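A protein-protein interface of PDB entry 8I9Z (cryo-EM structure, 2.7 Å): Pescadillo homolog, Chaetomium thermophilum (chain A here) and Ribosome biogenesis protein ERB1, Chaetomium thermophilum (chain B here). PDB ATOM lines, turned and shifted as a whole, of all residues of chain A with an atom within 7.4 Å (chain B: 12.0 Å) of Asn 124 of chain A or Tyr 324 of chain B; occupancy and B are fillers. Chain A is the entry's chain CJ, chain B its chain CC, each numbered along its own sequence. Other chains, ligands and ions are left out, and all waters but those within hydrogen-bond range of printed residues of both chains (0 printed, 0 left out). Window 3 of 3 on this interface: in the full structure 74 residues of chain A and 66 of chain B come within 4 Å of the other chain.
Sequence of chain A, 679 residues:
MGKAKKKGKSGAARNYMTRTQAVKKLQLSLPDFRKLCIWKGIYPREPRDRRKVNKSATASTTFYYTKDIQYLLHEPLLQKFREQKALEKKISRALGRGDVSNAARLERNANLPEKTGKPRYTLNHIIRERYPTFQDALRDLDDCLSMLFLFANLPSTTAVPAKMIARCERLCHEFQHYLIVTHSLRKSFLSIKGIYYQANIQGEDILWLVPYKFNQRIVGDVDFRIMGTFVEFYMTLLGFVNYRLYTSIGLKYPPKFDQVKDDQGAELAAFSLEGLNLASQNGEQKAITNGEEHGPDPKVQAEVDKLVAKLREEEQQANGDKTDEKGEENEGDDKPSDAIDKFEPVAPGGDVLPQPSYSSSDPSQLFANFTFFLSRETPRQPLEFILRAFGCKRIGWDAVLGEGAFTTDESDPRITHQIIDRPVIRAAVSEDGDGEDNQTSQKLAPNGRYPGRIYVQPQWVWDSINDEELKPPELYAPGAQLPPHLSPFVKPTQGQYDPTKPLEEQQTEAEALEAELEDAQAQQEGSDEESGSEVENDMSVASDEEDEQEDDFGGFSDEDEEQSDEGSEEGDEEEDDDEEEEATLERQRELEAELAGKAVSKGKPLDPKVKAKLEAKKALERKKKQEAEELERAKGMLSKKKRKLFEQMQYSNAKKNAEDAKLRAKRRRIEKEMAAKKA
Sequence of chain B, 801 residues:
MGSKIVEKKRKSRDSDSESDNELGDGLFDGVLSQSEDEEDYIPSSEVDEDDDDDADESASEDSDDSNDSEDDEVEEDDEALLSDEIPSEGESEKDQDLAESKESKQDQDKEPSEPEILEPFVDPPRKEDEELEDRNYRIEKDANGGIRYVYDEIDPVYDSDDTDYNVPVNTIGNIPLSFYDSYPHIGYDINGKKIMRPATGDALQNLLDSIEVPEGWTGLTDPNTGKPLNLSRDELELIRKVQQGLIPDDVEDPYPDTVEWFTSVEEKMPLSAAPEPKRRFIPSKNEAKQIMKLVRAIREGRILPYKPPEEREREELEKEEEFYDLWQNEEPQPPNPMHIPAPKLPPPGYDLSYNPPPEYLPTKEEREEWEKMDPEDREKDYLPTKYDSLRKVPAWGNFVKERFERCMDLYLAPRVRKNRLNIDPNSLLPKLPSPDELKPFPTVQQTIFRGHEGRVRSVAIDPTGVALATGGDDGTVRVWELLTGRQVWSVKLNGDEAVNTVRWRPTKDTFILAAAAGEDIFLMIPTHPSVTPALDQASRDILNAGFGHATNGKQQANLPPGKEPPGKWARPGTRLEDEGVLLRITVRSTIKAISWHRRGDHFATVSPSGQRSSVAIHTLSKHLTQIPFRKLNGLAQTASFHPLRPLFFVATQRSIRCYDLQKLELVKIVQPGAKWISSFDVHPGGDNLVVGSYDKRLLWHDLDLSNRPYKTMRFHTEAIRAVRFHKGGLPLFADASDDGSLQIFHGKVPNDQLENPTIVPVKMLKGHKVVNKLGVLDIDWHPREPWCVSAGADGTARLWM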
ATOM      1  N   PRO A 119     -29.940  -3.155  24.525  1.00  0.00           N
ATOM      2  CA  PRO A 119     -30.429  -2.693  25.829  1.00  0.00           C
ATOM      3  C   PRO A 119     -30.868  -1.238  25.800  1.00  0.00           C
ATOM      4  O   PRO A 119     -30.319  -0.413  25.066  1.00  0.00           O
ATOM      5  CB  PRO A 119     -29.216  -2.884  26.750  1.00  0.00           C
ATOM      6  CG  PRO A 119     -28.076  -3.223  25.861  1.00  0.00           C
ATOM      7  CD  PRO A 119     -28.674  -3.886  24.687  1.00  0.00           C
ATOM      8  N   TYR A 121     -30.745   1.007  28.256  1.00  0.00           N
ATOM      9  CA  TYR A 121     -29.818   1.883  28.946  1.00  0.00           C
ATOM     10  C   TYR A 121     -28.386   1.438  28.698  1.00  0.00           C
ATOM     11  O   TYR A 121     -28.084   0.242  28.676  1.00  0.00           O
ATOM     12  CB  TYR A 121     -30.107   1.904  30.448  1.00  0.00           C
ATOM     13  CG  TYR A 121     -31.516   2.321  30.779  1.00  0.00           C
ATOM     14  CD1 TYR A 121     -31.881   3.655  30.751  1.00  0.00           C
ATOM     15  CD2 TYR A 121     -32.486   1.383  31.094  1.00  0.00           C
ATOM     16  CE1 TYR A 121     -33.166   4.046  31.042  1.00  0.00           C
ATOM     17  CE2 TYR A 121     -33.778   1.765  31.382  1.00  0.00           C
ATOM     18  CZ  TYR A 121     -34.111   3.098  31.356  1.00  0.00           C
ATOM     19  OH  TYR A 121     -35.394   3.485  31.648  1.00  0.00           O
ATOM     20  N   THR A 122     -27.509   2.415  28.508  1.00  0.00           N
ATOM     21  CA  THR A 122     -26.086   2.148  28.350  1.00  0.00           C
ATOM     22  C   THR A 122     -25.508   1.689  29.683  1.00  0.00           C
ATOM     23  O   THR A 122     -25.483   2.452  30.653  1.00  0.00           O
ATOM     24  CB  THR A 122     -25.365   3.394  27.844  1.00  0.00           C
ATOM     25  OG1 THR A 122     -25.803   3.692  26.514  1.00  0.00           O
ATOM     26  CG2 THR A 122     -23.867   3.180  27.839  1.00  0.00           C
ATOM     27  N   LEU A 123     -25.052   0.440  29.730  1.00  0.00           N
ATOM     28  CA  LEU A 123     -24.527  -0.164  30.945  1.00  0.00           C
ATOM     29  C   LEU A 123     -23.009  -0.290  30.927  1.00  0.00           C
ATOM     30  O   LEU A 123     -22.456  -1.090  31.684  1.00  0.00           O
ATOM     31  CB  LEU A 123     -25.155  -1.539  31.163  1.00  0.00           C
ATOM     32  CG  LEU A 123     -26.537  -1.586  31.797  1.00  0.00           C
ATOM     33  CD1 LEU A 123     -27.376  -2.680  31.170  1.00  0.00           C
ATOM     34  CD2 LEU A 123     -26.391  -1.806  33.285  1.00  0.00           C
ATOM     35  N   ASN A 124     -22.329   0.477  30.072  1.00  0.00           N
ATOM     36  CA  ASN A 124     -20.890   0.309  29.889  1.00  0.00           C
ATOM     37  C   ASN A 124     -20.124   0.675  31.151  1.00  0.00           C
ATOM     38  O   ASN A 124     -19.158   0.002  31.523  1.00  0.00           O
ATOM     39  CB  ASN A 124     -20.408   1.153  28.710  1.00  0.00           C
ATOM     40  CG  ASN A 124     -21.209   0.909  27.457  1.00  0.00           C
ATOM     41  OD1 ASN A 124     -21.984  -0.039  27.377  1.00  0.00           O
ATOM     42  ND2 ASN A 124     -21.024   1.767  26.463  1.00  0.00           N
ATOM     43  N   HIS A 125     -20.546   1.743  31.823  1.00  0.00           N
ATOM     44  CA  HIS A 125     -19.854   2.178  33.029  1.00  0.00           C
ATOM     45  C   HIS A 125     -20.103   1.226  34.192  1.00  0.00           C
ATOM     46  O   HIS A 125     -19.227   1.042  35.039  1.00  0.00           O
ATOM     47  CB  HIS A 125     -20.264   3.607  33.399  1.00  0.00           C
ATOM     48  CG  HIS A 125     -21.726   3.787  33.684  1.00  0.00           C
ATOM     49  ND1 HIS A 125     -22.693   3.045  33.044  1.00  0.00           N
ATOM     50  CD2 HIS A 125     -22.387   4.600  34.543  1.00  0.00           C
ATOM     51  CE1 HIS A 125     -23.886   3.399  33.488  1.00  0.00           C
ATOM     52  NE2 HIS A 125     -23.727   4.343  34.398  1.00  0.00           N
ATOM     53  N   ILE A 126     -21.281   0.604  34.242  1.00  0.00           N
ATOM     54  CA  ILE A 126     -21.620  -0.277  35.357  1.00  0.00           C
ATOM     55  C   ILE A 126     -20.795  -1.557  35.305  1.00  0.00           C
ATOM     56  O   ILE A 126     -20.294  -2.031  36.333  1.00  0.00           O
ATOM     57  CB  ILE A 126     -23.134  -0.558  35.359  1.00  0.00           C
ATOM     58  CG1 ILE A 126     -23.884   0.639  35.945  1.00  0.00           C
ATOM     59  CG2 ILE A 126     -23.468  -1.830  36.120  1.00  0.00           C
ATOM     60  CD1 ILE A 126     -25.345   0.396  36.166  1.00  0.00           C
ATOM     61  N   ILE A 127     -20.616  -2.120  34.107  1.00  0.00           N
ATOM     62  CA  ILE A 127     -19.822  -3.338  33.951  1.00  0.00           C
ATOM     63  C   ILE A 127     -18.364  -3.080  34.317  1.00  0.00           C
ATOM     64  O   ILE A 127     -17.673  -3.963  34.839  1.00  0.00           O
ATOM     65  CB  ILE A 127     -19.970  -3.887  32.519  1.00  0.00           C
ATOM     66  CG1 ILE A 127     -21.437  -4.170  32.217  1.00  0.00           C
ATOM     67  CG2 ILE A 127     -19.177  -5.167  32.319  1.00  0.00           C
ATOM     68  CD1 ILE A 127     -21.754  -4.208  30.751  1.00  0.00           C
ATOM     69  N   ARG A 128     -17.884  -1.858  34.080  1.00  0.00           N
ATOM     70  CA  ARG A 128     -16.504  -1.527  34.415  1.00  0.00           C
ATOM     71  C   ARG A 128     -16.272  -1.521  35.924  1.00  0.00           C
ATOM     72  O   ARG A 128     -15.265  -2.054  36.401  1.00  0.00           O
ATOM     73  CB  ARG A 128     -16.127  -0.178  33.804  1.00  0.00           C
ATOM     74  CG  ARG A 128     -14.672   0.206  33.992  1.00  0.00           C
ATOM     75  CD  ARG A 128     -13.748  -0.900  33.518  1.00  0.00           C
ATOM     76  NE  ARG A 128     -12.415  -0.774  34.091  1.00  0.00           N
ATOM     77  CZ  ARG A 128     -11.422  -0.098  33.532  1.00  0.00           C
ATOM     78  NH1 ARG A 128     -11.572   0.515  32.371  1.00  0.00           N
ATOM     79  NH2 ARG A 128     -10.249  -0.034  34.155  1.00  0.00           N
ATOM     80  N   GLU A 129     -17.188  -0.925  36.696  1.00  0.00           N
ATOM     81  CA  GLU A 129     -17.030  -0.956  38.149  1.00  0.00           C
ATOM     82  C   GLU A 129     -17.336  -2.330  38.721  1.00  0.00           C
ATOM     83  O   GLU A 129     -16.797  -2.694  39.771  1.00  0.00           O
ATOM     84  CB  GLU A 129     -17.912   0.092  38.831  1.00  0.00           C
ATOM     85  CG  GLU A 129     -18.228   1.336  38.019  1.00  0.00           C
ATOM     86  CD  GLU A 129     -17.064   2.312  37.902  1.00  0.00           C
ATOM     87  OE1 GLU A 129     -15.998   2.075  38.509  1.00  0.00           O
ATOM     88  OE2 GLU A 129     -17.221   3.328  37.192  1.00  0.00           O
ATOM     89  N   ARG A 130     -18.193  -3.102  38.061  1.00  0.00           N
ATOM     90  CA  ARG A 130     -18.499  -4.434  38.562  1.00  0.00           C
ATOM     91  C   ARG A 130     -17.368  -5.414  38.273  1.00  0.00           C
ATOM     92  O   ARG A 130     -17.089  -6.301  39.087  1.00  0.00           O
ATOM     93  CB  ARG A 130     -19.811  -4.930  37.963  1.00  0.00           C
ATOM     94  CG  ARG A 130     -20.455  -6.016  38.779  1.00  0.00           C
ATOM     95  CD  ARG A 130     -21.910  -6.167  38.450  1.00  0.00           C
ATOM     96  NE  ARG A 130     -22.396  -7.469  38.874  1.00  0.00           N
ATOM     97  CZ  ARG A 130     -23.630  -7.907  38.677  1.00  0.00           C
ATOM     98  NH1 ARG A 130     -24.535  -7.166  38.064  1.00  0.00           N
ATOM     99  NH2 ARG A 130     -23.962  -9.120  39.106  1.00  0.00           N
ATOM    100  N   THR A 236     -24.849  -6.903  27.126  1.00  0.00           N
ATOM    101  CA  THR A 236     -23.812  -5.879  27.085  1.00  0.00           C
ATOM    102  C   THR A 236     -22.470  -6.427  27.554  1.00  0.00           C
ATOM    103  O   THR A 236     -21.416  -5.986  27.086  1.00  0.00           O
ATOM    104  CB  THR A 236     -24.230  -4.680  27.931  1.00  0.00           C
ATOM    105  OG1 THR A 236     -25.621  -4.418  27.729  1.00  0.00           O
ATOM    106  CG2 THR A 236     -23.446  -3.447  27.530  1.00  0.00           C
ATOM    107  N   GLY A 239     -20.906  -8.663  24.752  1.00  0.00           N
ATOM    108  CA  GLY A 239     -20.492  -7.879  23.601  1.00  0.00           C
ATOM    109  C   GLY A 239     -19.117  -7.268  23.777  1.00  0.00           C
ATOM    110  O   GLY A 239     -18.307  -7.244  22.848  1.00  0.00           O
ATOM    111  N   PHE A 240     -18.837  -6.759  24.974  1.00  0.00           N
ATOM    112  CA  PHE A 240     -17.519  -6.204  25.248  1.00  0.00           C
ATOM    113  C   PHE A 240     -16.492  -7.307  25.471  1.00  0.00           C
ATOM    114  O   PHE A 240     -15.296  -7.105  25.232  1.00  0.00           O
ATOM    115  CB  PHE A 240     -17.585  -5.276  26.457  1.00  0.00           C
ATOM    116  CG  PHE A 240     -18.138  -3.919  26.150  1.00  0.00           C
ATOM    117  CD1 PHE A 240     -17.411  -3.019  25.398  1.00  0.00           C
ATOM    118  CD2 PHE A 240     -19.376  -3.537  26.627  1.00  0.00           C
ATOM    119  CE1 PHE A 240     -17.914  -1.767  25.123  1.00  0.00           C
ATOM    120  CE2 PHE A 240     -19.882  -2.293  26.353  1.00  0.00           C
ATOM    121  CZ  PHE A 240     -19.152  -1.406  25.601  1.00  0.00           C
ATOM    122  N   VAL A 241     -16.935  -8.468  25.952  1.00  0.00           N
ATOM    123  CA  VAL A 241     -16.036  -9.608  26.104  1.00  0.00           C
ATOM    124  C   VAL A 241     -15.611 -10.131  24.739  1.00  0.00           C
ATOM    125  O   VAL A 241     -14.435 -10.445  24.514  1.00  0.00           O
ATOM    126  CB  VAL A 241     -16.706 -10.698  26.965  1.00  0.00           C
ATOM    127  CG1 VAL A 241     -16.104 -12.066  26.703  1.00  0.00           C
ATOM    128  CG2 VAL A 241     -16.579 -10.354  28.437  1.00  0.00           C
ATOM    129  N   TYR A 243     -15.441  -8.447  21.911  1.00  0.00           N
ATOM    130  CA  TYR A 243     -14.551  -7.506  21.238  1.00  0.00           C
ATOM    131  C   TYR A 243     -13.120  -7.661  21.730  1.00  0.00           C
ATOM    132  O   TYR A 243     -12.168  -7.581  20.946  1.00  0.00           O
ATOM    133  CB  TYR A 243     -15.030  -6.070  21.445  1.00  0.00           C
ATOM    134  CG  TYR A 243     -14.092  -5.040  20.856  1.00  0.00           C
ATOM    135  CD1 TYR A 243     -14.099  -4.769  19.500  1.00  0.00           C
ATOM    136  CD2 TYR A 243     -13.194  -4.347  21.656  1.00  0.00           C
ATOM    137  CE1 TYR A 243     -13.244  -3.839  18.958  1.00  0.00           C
ATOM    138  CE2 TYR A 243     -12.332  -3.422  21.119  1.00  0.00           C
ATOM    139  CZ  TYR A 243     -12.366  -3.170  19.772  1.00  0.00           C
ATOM    140  OH  TYR A 243     -11.510  -2.241  19.232  1.00  0.00           O
ATOM    141  N   ARG A 244     -12.952  -7.866  23.033  1.00  0.00           N
ATOM    142  CA  ARG A 244     -11.620  -8.035  23.595  1.00  0.00           C
ATOM    143  C   ARG A 244     -10.998  -9.348  23.131  1.00  0.00           C
ATOM    144  O   ARG A 244      -9.797  -9.417  22.852  1.00  0.00           O
ATOM    145  CB  ARG A 244     -11.703  -7.968  25.119  1.00  0.00           C
ATOM    146  CG  ARG A 244     -10.433  -8.332  25.847  1.00  0.00           C
ATOM    147  CD  ARG A 244      -9.615  -7.108  26.172  1.00  0.00           C
ATOM    148  NE  ARG A 244      -8.586  -7.430  27.147  1.00  0.00           N
ATOM    149  CZ  ARG A 244      -7.895  -6.534  27.833  1.00  0.00           C
ATOM    150  NH1 ARG A 244      -8.100  -5.236  27.677  1.00  0.00           N
ATOM    151  NH2 ARG A 244      -6.974  -6.949  28.698  1.00  0.00           N
ATOM    152  N   THR A 247     -10.115  -9.144  19.227  1.00  0.00           N
ATOM    153  CA  THR A 247      -8.958  -8.302  18.960  1.00  0.00           C
ATOM    154  C   THR A 247      -7.680  -8.958  19.462  1.00  0.00           C
ATOM    155  O   THR A 247      -6.584  -8.658  18.973  1.00  0.00           O
ATOM    156  CB  THR A 247      -9.159  -6.928  19.600  1.00  0.00           C
ATOM    157  OG1 THR A 247     -10.518  -6.521  19.420  1.00  0.00           O
ATOM    158  CG2 THR A 247      -8.259  -5.891  18.948  1.00  0.00           C
ATOM    159  N   TYR A 253     -13.977  -6.968  14.751  1.00  0.00           N
ATOM    160  CA  TYR A 253     -15.245  -7.134  15.427  1.00  0.00           C
ATOM    161  C   TYR A 253     -16.179  -5.992  15.053  1.00  0.00           C
ATOM    162  O   TYR A 253     -15.751  -4.835  15.011  1.00  0.00           O
ATOM    163  CB  TYR A 253     -15.057  -7.180  16.947  1.00  0.00           C
ATOM    164  CG  TYR A 253     -16.288  -7.644  17.672  1.00  0.00           C
ATOM    165  CD1 TYR A 253     -16.599  -8.990  17.745  1.00  0.00           C
ATOM    166  CD2 TYR A 253     -17.153  -6.737  18.263  1.00  0.00           C
ATOM    167  CE1 TYR A 253     -17.725  -9.421  18.393  1.00  0.00           C
ATOM    168  CE2 TYR A 253     -18.285  -7.159  18.914  1.00  0.00           C
ATOM    169  CZ  TYR A 253     -18.566  -8.503  18.978  1.00  0.00           C
ATOM    170  OH  TYR A 253     -19.698  -8.931  19.627  1.00  0.00           O
ATOM    171  N   PHE B 323     -17.757   0.008  18.605  1.00  0.00           N
ATOM    172  CA  PHE B 323     -17.255  -0.865  19.660  1.00  0.00           C
ATOM    173  C   PHE B 323     -15.883  -0.424  20.145  1.00  0.00           C
ATOM    174  O   PHE B 323     -15.104   0.152  19.389  1.00  0.00           O
ATOM    175  CB  PHE B 323     -17.189  -2.314  19.177  1.00  0.00           C
ATOM    176  CG  PHE B 323     -18.530  -2.919  18.884  1.00  0.00           C
ATOM    177  CD1 PHE B 323     -19.048  -2.900  17.603  1.00  0.00           C
ATOM    178  CD2 PHE B 323     -19.270  -3.510  19.895  1.00  0.00           C
ATOM    179  CE1 PHE B 323     -20.284  -3.458  17.331  1.00  0.00           C
ATOM    180  CE2 PHE B 323     -20.506  -4.070  19.632  1.00  0.00           C
ATOM    181  CZ  PHE B 323     -21.014  -4.044  18.348  1.00  0.00           C
ATOM    182  N   TYR B 324     -15.595  -0.700  21.412  1.00  0.00           N
ATOM    183  CA  TYR B 324     -14.318  -0.330  22.003  1.00  0.00           C
ATOM    184  C   TYR B 324     -14.037  -1.253  23.179  1.00  0.00           C
ATOM    185  O   TYR B 324     -14.912  -1.984  23.646  1.00  0.00           O
ATOM    186  CB  TYR B 324     -14.301   1.141  22.430  1.00  0.00           C
ATOM    187  CG  TYR B 324     -15.202   1.480  23.594  1.00  0.00           C
ATOM    188  CD1 TYR B 324     -16.559   1.704  23.404  1.00  0.00           C
ATOM    189  CD2 TYR B 324     -14.693   1.607  24.877  1.00  0.00           C
ATOM    190  CE1 TYR B 324     -17.383   2.021  24.462  1.00  0.00           C
ATOM    191  CE2 TYR B 324     -15.510   1.923  25.941  1.00  0.00           C
ATOM    192  CZ  TYR B 324     -16.854   2.130  25.726  1.00  0.00           C
ATOM    193  OH  TYR B 324     -17.671   2.449  26.785  1.00  0.00           O
ATOM    194  N   ASP B 325     -12.794  -1.212  23.645  1.00  0.00           N
ATOM    195  CA  ASP B 325     -12.344  -2.038  24.756  1.00  0.00           C
ATOM    196  C   ASP B 325     -12.642  -1.291  26.051  1.00  0.00           C
ATOM    197  O   ASP B 325     -12.222  -0.142  26.218  1.00  0.00           O
ATOM    198  CB  ASP B 325     -10.847  -2.329  24.615  1.00  0.00           C
ATOM    199  CG  ASP B 325     -10.312  -3.297  25.664  1.00  0.00           C
ATOM    200  OD1 ASP B 325     -11.050  -3.721  26.579  1.00  0.00           O
ATOM    201  OD2 ASP B 325      -9.116  -3.643  25.568  1.00  0.00           O
ATOM    202  N   LEU B 326     -13.376  -1.940  26.958  1.00  0.00           N
ATOM    203  CA  LEU B 326     -13.664  -1.328  28.252  1.00  0.00           C
ATOM    204  C   LEU B 326     -12.404  -1.189  29.089  1.00  0.00           C
ATOM    205  O   LEU B 326     -12.209  -0.175  29.769  1.00  0.00           O
ATOM    206  CB  LEU B 326     -14.707  -2.146  29.007  1.00  0.00           C
ATOM    207  CG  LEU B 326     -16.171  -1.937  28.637  1.00  0.00           C
ATOM    208  CD1 LEU B 326     -17.046  -2.903  29.414  1.00  0.00           C
ATOM    209  CD2 LEU B 326     -16.584  -0.501  28.902  1.00  0.00           C
ATOM    210  N   TRP B 327     -11.539  -2.195  29.054  1.00  0.00           N
ATOM    211  CA  TRP B 327     -10.335  -2.222  29.879  1.00  0.00           C
ATOM    212  C   TRP B 327      -9.128  -1.657  29.139  1.00  0.00           C
ATOM    213  O   TRP B 327      -8.099  -2.317  28.998  1.00  0.00           O
ATOM    214  CB  TRP B 327     -10.077  -3.646  30.350  1.00  0.00           C
ATOM    215  CG  TRP B 327     -11.273  -4.285  30.978  1.00  0.00           C
ATOM    216  CD1 TRP B 327     -11.584  -4.311  32.303  1.00  0.00           C
ATOM    217  CD2 TRP B 327     -12.317  -4.997  30.308  1.00  0.00           C
ATOM    218  NE1 TRP B 327     -12.757  -4.990  32.501  1.00  0.00           N
ATOM    219  CE2 TRP B 327     -13.227  -5.422  31.290  1.00  0.00           C
ATOM    220  CE3 TRP B 327     -12.570  -5.314  28.972  1.00  0.00           C
ATOM    221  CZ2 TRP B 327     -14.368  -6.148  30.981  1.00  0.00           C
ATOM    222  CZ3 TRP B 327     -13.706  -6.034  28.668  1.00  0.00           C
ATOM    223  CH2 TRP B 327     -14.591  -6.442  29.665  1.00  0.00           C
ATOM    224  N   GLN B 328      -9.250  -0.423  28.647  1.00  0.00           N
ATOM    225  CA  GLN B 328      -8.106   0.238  28.029  1.00  0.00           C
ATOM    226  C   GLN B 328      -7.055   0.594  29.070  1.00  0.00           C
ATOM    227  O   GLN B 328      -5.856   0.394  28.847  1.00  0.00           O
ATOM    228  CB  GLN B 328      -8.560   1.490  27.279  1.00  0.00           C
ATOM    229  CG  GLN B 328      -9.218   1.215  25.939  1.00  0.00           C
ATOM    230  CD  GLN B 328      -9.693   2.480  25.251  1.00  0.00           C
ATOM    231  OE1 GLN B 328      -9.597   3.575  25.807  1.00  0.00           O
ATOM    232  NE2 GLN B 328     -10.208   2.337  24.036  1.00  0.00           N
ATOM    233  N   ASN B 329      -7.484   1.121  30.211  1.00  0.00           N
ATOM    234  CA  ASN B 329      -6.608   1.436  31.335  1.00  0.00           C
ATOM    235  C   ASN B 329      -6.956   0.444  32.437  1.00  0.00           C
ATOM    236  O   ASN B 329      -7.801   0.712  33.293  1.00  0.00           O
ATOM    237  CB  ASN B 329      -6.776   2.877  31.789  1.00  0.00           C
ATOM    238  CG  ASN B 329      -6.346   3.873  30.733  1.00  0.00           C
ATOM    239  OD1 ASN B 329      -7.162   4.631  30.208  1.00  0.00           O
ATOM    240  ND2 ASN B 329      -5.058   3.877  30.414  1.00  0.00           N
ATOM    241  N   GLU B 330      -6.293  -0.703  32.411  1.00  0.00           N
ATOM    242  CA  GLU B 330      -6.622  -1.831  33.269  1.00  0.00           C
ATOM    243  C   GLU B 330      -5.560  -1.951  34.354  1.00  0.00           C
ATOM    244  O   GLU B 330      -4.381  -2.158  34.052  1.00  0.00           O
ATOM    245  CB  GLU B 330      -6.701  -3.106  32.432  1.00  0.00           C
ATOM    246  CG  GLU B 330      -7.293  -4.315  33.114  1.00  0.00           C
ATOM    247  CD  GLU B 330      -7.103  -5.566  32.282  1.00  0.00           C
ATOM    248  OE1 GLU B 330      -6.101  -5.635  31.542  1.00  0.00           O
ATOM    249  OE2 GLU B 330      -7.969  -6.463  32.333  1.00  0.00           O
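OD1 of Asp 325 of chain B lies within hydrogen-bond range of N of Trp 327 of chain B (2.9 Å).
OG1 of Thr 247 of chain A lies within hydrogen-bond range of O of Tyr 243 of chain A, 2.5 Å away.
The side-chain carboxylate (OD2) of Asp 325 of chain B is in salt-bridge range of the guanidinium group (NH1) of Arg 244 of chain A, 2.8 Å away.
O of Trp 327 of chain B is in hydrogen-bond range of NH1 of Arg 244 of chain A (3.2 Å).
The guanidinium group of Arg 128 of chain A lies within hydrogen-bond range of the backbone carbonyl oxygen of Leu 326 of chain B.
The side-chain amide nitrogen of Asn 124 of chain A lies within hydrogen-bond range of the side-chain hydroxyl of Tyr 324 of chain B, at 3.4 Å.
OE1 of Glu 330 of chain B lies within salt-bridge range of NH2 of Arg 244 of chain A.
O of Asn 329 of chain B sits at hydrogen-bond distance from NH2 of Arg 128 of chain A.
Of chain B, only Tyr 324 and Leu 326 come within 4 Å of Asn 124 of chain A.
Tyr 324 of chain B touches just these residues of chain A: Asn 124, Phe 240 and Tyr 243.
No residue of chain B comes within 4 Å of Leu 123 of chain A.
No residue of chain B comes within 4 Å of His 125 of chain A.
No residue of chain B comes within 4 Å of Ile 127 of chain A.
No residue of chain B comes within 4 Å of Thr 236 of chain A.
Of the printed residues of chain B, Phe 240 of chain A touches Tyr 324 (3.2 Å), Leu 326 (3.6 Å) and Trp 327 (3.9 Å).
Of chain B, only Phe 323, Tyr 324 and Asp 325 come within 4 Å of Tyr 243 of chain A.
Printed residues of chain A within 4 Å of Glu 330 of chain B: Arg 244.
Printed residues of chain A within 4 Å of Asp 325 of chain B: Tyr 243 and Arg 244.
Of the printed residues of chain B, Tyr 253 of chain A touches Phe 323.
The nearest residue of chain A that does not touch Tyr 324 of chain B is His 125 of chain A (5.8 Å).
Asn 124 of chain A touches Leu 326 of chain B.
Arg 128 of chain A touches Trp 327 of chain B.
O of Tyr 324 of chain B touches CD1 of Phe 240 of chain A (3.2 Å).
Leu 326 of chain B touches Phe 240 of chain A.
Trp 327 of chain B touches Phe 240 of chain A.
Phe 323 of chain B touches Tyr 243 of chain A.
Tyr 243 of chain A touches Tyr 324 of chain B (CE2 to C, 3.4 Å).
CE2 of Tyr 243 of chain A touches N of Asp 325 of chain B, at 3.4 Å.
CE2 of Tyr 253 of chain A touches CE2 of Phe 323 of chain B, 3.9 Å away.
Of the 8 printed residues of chain B, 7 touch a printed residue of chain A.
Among the printed residues, Asp or Glu carboxylates within 4 Å of a Lys or Arg side-chain nitrogen of the other chain: Arg 244 of chain A with Asp 325 of chain B (2.8 Å) and Arg 244 of chain A with Glu 330 of chain B (3.3 Å).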
